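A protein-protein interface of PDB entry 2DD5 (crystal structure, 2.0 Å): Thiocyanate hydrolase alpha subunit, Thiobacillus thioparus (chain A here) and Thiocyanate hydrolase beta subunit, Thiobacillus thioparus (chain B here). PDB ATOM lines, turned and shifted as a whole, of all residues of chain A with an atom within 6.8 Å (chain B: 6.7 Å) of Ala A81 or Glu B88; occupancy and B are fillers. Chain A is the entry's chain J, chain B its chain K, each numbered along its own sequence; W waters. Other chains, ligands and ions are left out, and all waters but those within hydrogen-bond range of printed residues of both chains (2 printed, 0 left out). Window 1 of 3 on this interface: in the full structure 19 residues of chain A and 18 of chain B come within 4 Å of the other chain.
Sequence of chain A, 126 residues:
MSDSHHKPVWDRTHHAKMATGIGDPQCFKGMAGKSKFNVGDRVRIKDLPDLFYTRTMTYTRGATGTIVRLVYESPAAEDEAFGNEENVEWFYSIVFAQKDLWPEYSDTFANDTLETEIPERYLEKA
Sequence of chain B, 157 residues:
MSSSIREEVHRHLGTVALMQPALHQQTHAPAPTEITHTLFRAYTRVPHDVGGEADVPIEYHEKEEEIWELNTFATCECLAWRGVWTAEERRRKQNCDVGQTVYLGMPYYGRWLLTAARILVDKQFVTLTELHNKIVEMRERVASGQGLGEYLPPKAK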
ATOM      1  N   TYR A  53       8.778  -4.085  19.343  1.00  0.00           N
ATOM      2  CA  TYR A  53      10.225  -3.998  19.520  1.00  0.00           C
ATOM      3  C   TYR A  53      11.009  -3.521  18.301  1.00  0.00           C
ATOM      4  O   TYR A  53      10.641  -3.786  17.158  1.00  0.00           O
ATOM      5  CB  TYR A  53      10.776  -5.368  19.938  1.00  0.00           C
ATOM      6  CG  TYR A  53      12.174  -5.324  20.520  1.00  0.00           C
ATOM      7  CD1 TYR A  53      12.431  -4.630  21.698  1.00  0.00           C
ATOM      8  CD2 TYR A  53      13.236  -5.984  19.899  1.00  0.00           C
ATOM      9  CE1 TYR A  53      13.705  -4.590  22.250  1.00  0.00           C
ATOM     10  CE2 TYR A  53      14.522  -5.951  20.447  1.00  0.00           C
ATOM     11  CZ  TYR A  53      14.745  -5.252  21.625  1.00  0.00           C
ATOM     12  OH  TYR A  53      15.998  -5.217  22.194  1.00  0.00           O
ATOM     13  N   ARG A  55      15.385  -1.784  17.627  1.00  0.00           N
ATOM     14  CA  ARG A  55      16.572  -1.185  18.217  1.00  0.00           C
ATOM     15  C   ARG A  55      17.102  -0.082  17.300  1.00  0.00           C
ATOM     16  O   ARG A  55      18.254   0.330  17.401  1.00  0.00           O
ATOM     17  CB  ARG A  55      17.650  -2.238  18.514  1.00  0.00           C
ATOM     18  CG  ARG A  55      17.243  -3.212  19.632  1.00  0.00           C
ATOM     19  CD  ARG A  55      18.420  -4.032  20.147  1.00  0.00           C
ATOM     20  NE  ARG A  55      19.346  -3.231  20.952  1.00  0.00           N
ATOM     21  CZ  ARG A  55      19.101  -2.824  22.196  1.00  0.00           C
ATOM     22  NH1 ARG A  55      17.956  -3.141  22.790  1.00  0.00           N
ATOM     23  NH2 ARG A  55      20.004  -2.110  22.852  1.00  0.00           N
ATOM     24  N   ALA A  76      18.752  -9.828  13.100  1.00  0.00           N
ATOM     25  CA  ALA A  76      18.279  -8.524  13.554  1.00  0.00           C
ATOM     26  C   ALA A  76      17.742  -8.685  14.976  1.00  0.00           C
ATOM     27  O   ALA A  76      17.138  -9.710  15.300  1.00  0.00           O
ATOM     28  CB  ALA A  76      17.174  -8.016  12.638  1.00  0.00           C
ATOM     29  N   ALA A  77      17.961  -7.683  15.820  1.00  0.00           N
ATOM     30  CA  ALA A  77      17.481  -7.741  17.199  1.00  0.00           C
ATOM     31  C   ALA A  77      15.976  -7.991  17.225  1.00  0.00           C
ATOM     32  O   ALA A  77      15.465  -8.641  18.136  1.00  0.00           O
ATOM     33  CB  ALA A  77      17.809  -6.441  17.924  1.00  0.00           C
ATOM     34  N   GLU A  78      15.273  -7.474  16.219  1.00  0.00           N
ATOM     35  CA  GLU A  78      13.830  -7.647  16.126  1.00  0.00           C
ATOM     36  C   GLU A  78      13.454  -9.131  16.036  1.00  0.00           C
ATOM     37  O   GLU A  78      12.346  -9.521  16.404  1.00  0.00           O
ATOM     38  CB  GLU A  78      13.279  -6.898  14.906  1.00  0.00           C
ATOM     39  CG  GLU A  78      13.335  -5.365  14.985  1.00  0.00           C
ATOM     40  CD  GLU A  78      14.749  -4.794  14.898  1.00  0.00           C
ATOM     41  OE1 GLU A  78      15.688  -5.542  14.553  1.00  0.00           O
ATOM     42  OE2 GLU A  78      14.921  -3.583  15.164  1.00  0.00           O
ATOM     43  N   ASP A  79      14.370  -9.955  15.535  1.00  0.00           N
ATOM     44  CA  ASP A  79      14.112 -11.389  15.433  1.00  0.00           C
ATOM     45  C   ASP A  79      14.711 -12.120  16.628  1.00  0.00           C
ATOM     46  O   ASP A  79      14.079 -12.990  17.225  1.00  0.00           O
ATOM     47  CB  ASP A  79      14.704 -11.966  14.142  1.00  0.00           C
ATOM     48  CG  ASP A  79      13.934 -11.538  12.903  1.00  0.00           C
ATOM     49  OD1 ASP A  79      12.691 -11.439  12.980  1.00  0.00           O
ATOM     50  OD2 ASP A  79      14.571 -11.317  11.852  1.00  0.00           O
ATOM     51  N   GLU A  80      15.935 -11.745  16.973  1.00  0.00           N
ATOM     52  CA  GLU A  80      16.651 -12.354  18.083  1.00  0.00           C
ATOM     53  C   GLU A  80      15.877 -12.219  19.400  1.00  0.00           C
ATOM     54  O   GLU A  80      15.824 -13.155  20.198  1.00  0.00           O
ATOM     55  CB  GLU A  80      18.031 -11.701  18.199  1.00  0.00           C
ATOM     56  CG  GLU A  80      19.088 -12.526  18.907  1.00  0.00           C
ATOM     57  CD  GLU A  80      20.481 -11.937  18.727  1.00  0.00           C
ATOM     58  OE1 GLU A  80      20.699 -10.785  19.163  1.00  0.00           O
ATOM     59  OE2 GLU A  80      21.354 -12.618  18.147  1.00  0.00           O
ATOM     60  N   ALA A  81      15.264 -11.059  19.613  1.00  0.00           N
ATOM     61  CA  ALA A  81      14.502 -10.796  20.832  1.00  0.00           C
ATOM     62  C   ALA A  81      13.275 -11.693  20.982  1.00  0.00           C
ATOM     63  O   ALA A  81      12.664 -11.734  22.049  1.00  0.00           O
ATOM     64  CB  ALA A  81      14.077  -9.329  20.876  1.00  0.00           C
ATOM     65  N   PHE A  82      12.912 -12.405  19.919  1.00  0.00           N
ATOM     66  CA  PHE A  82      11.762 -13.301  19.967  1.00  0.00           C
ATOM     67  C   PHE A  82      12.134 -14.750  19.670  1.00  0.00           C
ATOM     68  O   PHE A  82      11.271 -15.576  19.353  1.00  0.00           O
ATOM     69  CB  PHE A  82      10.670 -12.801  19.018  1.00  0.00           C
ATOM     70  CG  PHE A  82       9.932 -11.600  19.547  1.00  0.00           C
ATOM     71  CD1 PHE A  82       8.912 -11.751  20.482  1.00  0.00           C
ATOM     72  CD2 PHE A  82      10.304 -10.315  19.165  1.00  0.00           C
ATOM     73  CE1 PHE A  82       8.274 -10.638  21.033  1.00  0.00           C
ATOM     74  CE2 PHE A  82       9.675  -9.198  19.710  1.00  0.00           C
ATOM     75  CZ  PHE A  82       8.660  -9.357  20.644  1.00  0.00           C
ATOM     76  N   GLY A  83      13.426 -15.045  19.791  1.00  0.00           N
ATOM     77  CA  GLY A  83      13.926 -16.393  19.575  1.00  0.00           C
ATOM     78  C   GLY A  83      14.044 -16.855  18.136  1.00  0.00           C
ATOM     79  O   GLY A  83      14.107 -18.059  17.875  1.00  0.00           O
ATOM     80  N   ASN A  84      14.084 -15.912  17.199  1.00  0.00           N
ATOM     81  CA  ASN A  84      14.181 -16.253  15.782  1.00  0.00           C
ATOM     82  C   ASN A  84      15.556 -15.842  15.259  1.00  0.00           C
ATOM     83  O   ASN A  84      15.828 -14.656  15.082  1.00  0.00           O
ATOM     84  CB  ASN A  84      13.079 -15.530  14.995  1.00  0.00           C
ATOM     85  CG  ASN A  84      11.681 -15.797  15.551  1.00  0.00           C
ATOM     86  OD1 ASN A  84      10.905 -14.866  15.789  1.00  0.00           O
ATOM     87  ND2 ASN A  84      11.356 -17.066  15.754  1.00  0.00           N
ATOM     88  N   TRP B  85      17.573 -17.885  27.928  1.00  0.00           N
ATOM     89  CA  TRP B  85      17.267 -16.766  27.040  1.00  0.00           C
ATOM     90  C   TRP B  85      18.557 -16.122  26.562  1.00  0.00           C
ATOM     91  O   TRP B  85      19.642 -16.473  27.020  1.00  0.00           O
ATOM     92  CB  TRP B  85      16.400 -15.709  27.749  1.00  0.00           C
ATOM     93  CG  TRP B  85      17.017 -15.042  28.973  1.00  0.00           C
ATOM     94  CD1 TRP B  85      18.262 -15.251  29.497  1.00  0.00           C
ATOM     95  CD2 TRP B  85      16.382 -14.080  29.829  1.00  0.00           C
ATOM     96  NE1 TRP B  85      18.440 -14.481  30.627  1.00  0.00           N
ATOM     97  CE2 TRP B  85      17.301 -13.755  30.852  1.00  0.00           C
ATOM     98  CE3 TRP B  85      15.124 -13.460  29.829  1.00  0.00           C
ATOM     99  CZ2 TRP B  85      17.000 -12.837  31.873  1.00  0.00           C
ATOM    100  CZ3 TRP B  85      14.823 -12.549  30.842  1.00  0.00           C
ATOM    101  CH2 TRP B  85      15.759 -12.248  31.849  1.00  0.00           C
ATOM    102  N   THR B  86      18.433 -15.202  25.614  1.00  0.00           N
ATOM    103  CA  THR B  86      19.585 -14.465  25.113  1.00  0.00           C
ATOM    104  C   THR B  86      19.398 -13.069  25.681  1.00  0.00           C
ATOM    105  O   THR B  86      18.295 -12.721  26.104  1.00  0.00           O
ATOM    106  CB  THR B  86      19.591 -14.372  23.578  1.00  0.00           C
ATOM    107  OG1 THR B  86      18.362 -13.781  23.135  1.00  0.00           O
ATOM    108  CG2 THR B  86      19.751 -15.758  22.959  1.00  0.00           C
ATOM    109  N   ALA B  87      20.462 -12.271  25.695  1.00  0.00           N
ATOM    110  CA  ALA B  87      20.368 -10.919  26.224  1.00  0.00           C
ATOM    111  C   ALA B  87      19.318 -10.107  25.473  1.00  0.00           C
ATOM    112  O   ALA B  87      18.640  -9.270  26.065  1.00  0.00           O
ATOM    113  CB  ALA B  87      21.732 -10.220  26.146  1.00  0.00           C
ATOM    114  N   GLU B  88      19.180 -10.350  24.173  1.00  0.00           N
ATOM    115  CA  GLU B  88      18.194  -9.611  23.394  1.00  0.00           C
ATOM    116  C   GLU B  88      16.768  -9.903  23.837  1.00  0.00           C
ATOM    117  O   GLU B  88      15.926  -9.001  23.868  1.00  0.00           O
ATOM    118  CB  GLU B  88      18.362  -9.888  21.897  1.00  0.00           C
ATOM    119  CG  GLU B  88      19.211  -8.821  21.228  1.00  0.00           C
ATOM    120  CD  GLU B  88      18.688  -7.420  21.533  1.00  0.00           C
ATOM    121  OE1 GLU B  88      19.482  -6.561  21.971  1.00  0.00           O
ATOM    122  OE2 GLU B  88      17.475  -7.185  21.341  1.00  0.00           O
ATOM    123  N   GLU B  89      16.491 -11.160  24.171  1.00  0.00           N
ATOM    124  CA  GLU B  89      15.167 -11.523  24.655  1.00  0.00           C
ATOM    125  C   GLU B  89      14.960 -10.806  25.989  1.00  0.00           C
ATOM    126  O   GLU B  89      13.871 -10.298  26.266  1.00  0.00           O
ATOM    127  CB  GLU B  89      15.060 -13.035  24.869  1.00  0.00           C
ATOM    128  CG  GLU B  89      15.007 -13.848  23.590  1.00  0.00           C
ATOM    129  CD  GLU B  89      14.995 -15.343  23.858  1.00  0.00           C
ATOM    130  OE1 GLU B  89      16.009 -15.865  24.365  1.00  0.00           O
ATOM    131  OE2 GLU B  89      13.968 -15.993  23.568  1.00  0.00           O
ATOM    132  N   ARG B  90      16.008 -10.764  26.812  1.00  0.00           N
ATOM    133  CA  ARG B  90      15.916 -10.085  28.101  1.00  0.00           C
ATOM    134  C   ARG B  90      15.589  -8.604  27.924  1.00  0.00           C
ATOM    135  O   ARG B  90      14.672  -8.081  28.559  1.00  0.00           O
ATOM    136  CB  ARG B  90      17.222 -10.208  28.893  1.00  0.00           C
ATOM    137  CG  ARG B  90      17.215  -9.363  30.181  1.00  0.00           C
ATOM    138  CD  ARG B  90      18.502  -9.505  30.998  1.00  0.00           C
ATOM    139  NE  ARG B  90      19.693  -9.050  30.277  1.00  0.00           N
ATOM    140  CZ  ARG B  90      19.945  -7.789  29.933  1.00  0.00           C
ATOM    141  NH1 ARG B  90      19.092  -6.816  30.238  1.00  0.00           N
ATOM    142  NH2 ARG B  90      21.061  -7.503  29.271  1.00  0.00           N
ATOM    143  N   ARG B  91      16.338  -7.926  27.059  1.00  0.00           N
ATOM    144  CA  ARG B  91      16.107  -6.499  26.836  1.00  0.00           C
ATOM    145  C   ARG B  91      14.675  -6.206  26.406  1.00  0.00           C
ATOM    146  O   ARG B  91      14.041  -5.291  26.928  1.00  0.00           O
ATOM    147  CB  ARG B  91      17.085  -5.948  25.790  1.00  0.00           C
ATOM    148  CG  ARG B  91      18.530  -5.926  26.265  1.00  0.00           C
ATOM    149  CD  ARG B  91      19.453  -5.145  25.323  1.00  0.00           C
ATOM    150  NE  ARG B  91      20.836  -5.275  25.776  1.00  0.00           N
ATOM    151  CZ  ARG B  91      21.655  -6.254  25.402  1.00  0.00           C
ATOM    152  NH1 ARG B  91      21.241  -7.178  24.545  1.00  0.00           N
ATOM    153  NH2 ARG B  91      22.866  -6.349  25.938  1.00  0.00           N
ATOM    154  N   ARG B  92      14.170  -6.984  25.457  1.00  0.00           N
ATOM    155  CA  ARG B  92      12.809  -6.794  24.964  1.00  0.00           C
ATOM    156  C   ARG B  92      11.783  -6.920  26.099  1.00  0.00           C
ATOM    157  O   ARG B  92      10.890  -6.087  26.235  1.00  0.00           O
ATOM    158  CB  ARG B  92      12.526  -7.811  23.848  1.00  0.00           C
ATOM    159  CG  ARG B  92      11.135  -7.724  23.234  1.00  0.00           C
ATOM    160  CD  ARG B  92      10.190  -8.726  23.877  1.00  0.00           C
ATOM    161  NE  ARG B  92      10.612 -10.104  23.633  1.00  0.00           N
ATOM    162  CZ  ARG B  92       9.962 -11.177  24.080  1.00  0.00           C
ATOM    163  NH1 ARG B  92       8.857 -11.031  24.798  1.00  0.00           N
ATOM    164  NH2 ARG B  92      10.410 -12.396  23.805  1.00  0.00           N
ATOM    165  N   LYS B  93      11.918  -7.956  26.921  1.00  0.00           N
ATOM    166  CA  LYS B  93      10.990  -8.167  28.033  1.00  0.00           C
ATOM    167  C   LYS B  93      11.188  -7.150  29.152  1.00  0.00           C
ATOM    168  O   LYS B  93      10.232  -6.644  29.732  1.00  0.00           O
ATOM    169  CB  LYS B  93      11.182  -9.571  28.622  1.00  0.00           C
ATOM    170  CG  LYS B  93      10.953 -10.720  27.645  1.00  0.00           C
ATOM    171  CD  LYS B  93      11.341 -12.061  28.270  1.00  0.00           C
ATOM    172  CE  LYS B  93      10.389 -12.460  29.391  1.00  0.00           C
ATOM    173  NZ  LYS B  93       9.015 -12.695  28.879  1.00  0.00           N
HETATM  174  O   HOH W   1      21.510 -11.412  22.313  1.00  0.00           O
HETATM  175  O   HOH W   2      17.333 -15.203  20.737  1.00  0.00           O
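Of the 9 printed residues of chain B, 5 touch a printed residue of chain A. Of the 11 printed residues of chain A, 7 touch a printed residue of chain B. Among the printed residues, 14 pairs touch across the chains. Among the printed residues, Asp or Glu carboxylates within 4 Å of a Lys or Arg side-chain nitrogen of the other chain: Arg A55 with Glu B88.
Arg B91 touches Tyr A53. CE1 of Tyr A53 touches CA of Arg B92 (3.6 Å). Arg B91 touches Arg A55. CB of Ala A77 touches OE2 of Glu B88 (3.5 Å). Thr B86 touches Glu A80. Glu B88 touches Glu A80 (CG to OE1, 3.2 Å). O of Glu A80 touches CG of Glu B89, 3.6 Å away. Ala A81 touches Glu B88 (CB to O, 3.5 Å). Arg B92 touches Phe A82. Glu B89 touches Gly A83 (OE2 to N, 3.9 Å).
Water W2 lies within hydrogen-bond range of the backbone carbonyl oxygen of Glu A80 (2.6 Å) and the side-chain hydroxyl of Thr B86 (3.0 Å). Water W1 bridges N of Glu B88 (3.2 Å) and OE1 of Glu A80 (3.3 Å).
OH of Tyr A53 sits at hydrogen-bond distance from OE2 of Glu B88 (2.6 Å). The guanidinium group (NE) of Arg A55 lies within salt-bridge range of the side-chain carboxylate (OE1) of Glu B88, at 3.5 Å. The backbone carbonyl oxygen of Ala A81 sits at hydrogen-bond distance from the guanidinium group of Arg B92, 2.9 Å away.
NH1 of Arg A55 lies within hydrogen-bond range of OH of Tyr A53 (2.9 Å). N of Arg A55 sits at hydrogen-bond distance from OE2 of Glu A78 (3.1 Å). The backbone NH of Thr B86 sits at hydrogen-bond distance from the side-chain carboxylate of Glu B89 (2.8 Å). The side-chain carboxylate of Glu B88 lies within salt-bridge range of the guanidinium group of Arg B91 (3.2 Å).
Printed residues of chain A within 4 Å of Glu B88: Tyr A53, Arg A55, Ala A77, Glu A80 and Ala A81. Printed residues of chain A within 4 Å of Glu B89: Glu A80, Ala A81 and Gly A83. Of the printed residues of chain B, Ala A77 touches Glu B88. Of the printed residues of chain B, Gly A83 touches Glu B89 (3.9 Å). Of the printed residues of chain B, Glu A80 touches Thr B86 (3.9 Å), Glu B88 (3.2 Å) and Glu B89 (3.6 Å). Of the printed residues of chain B, Tyr A53 touches Glu B88, Arg B91 and Arg B92. Arg B90 touches none of the printed residues of chain A. Asn A84 touches none of the printed residues of chain B.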
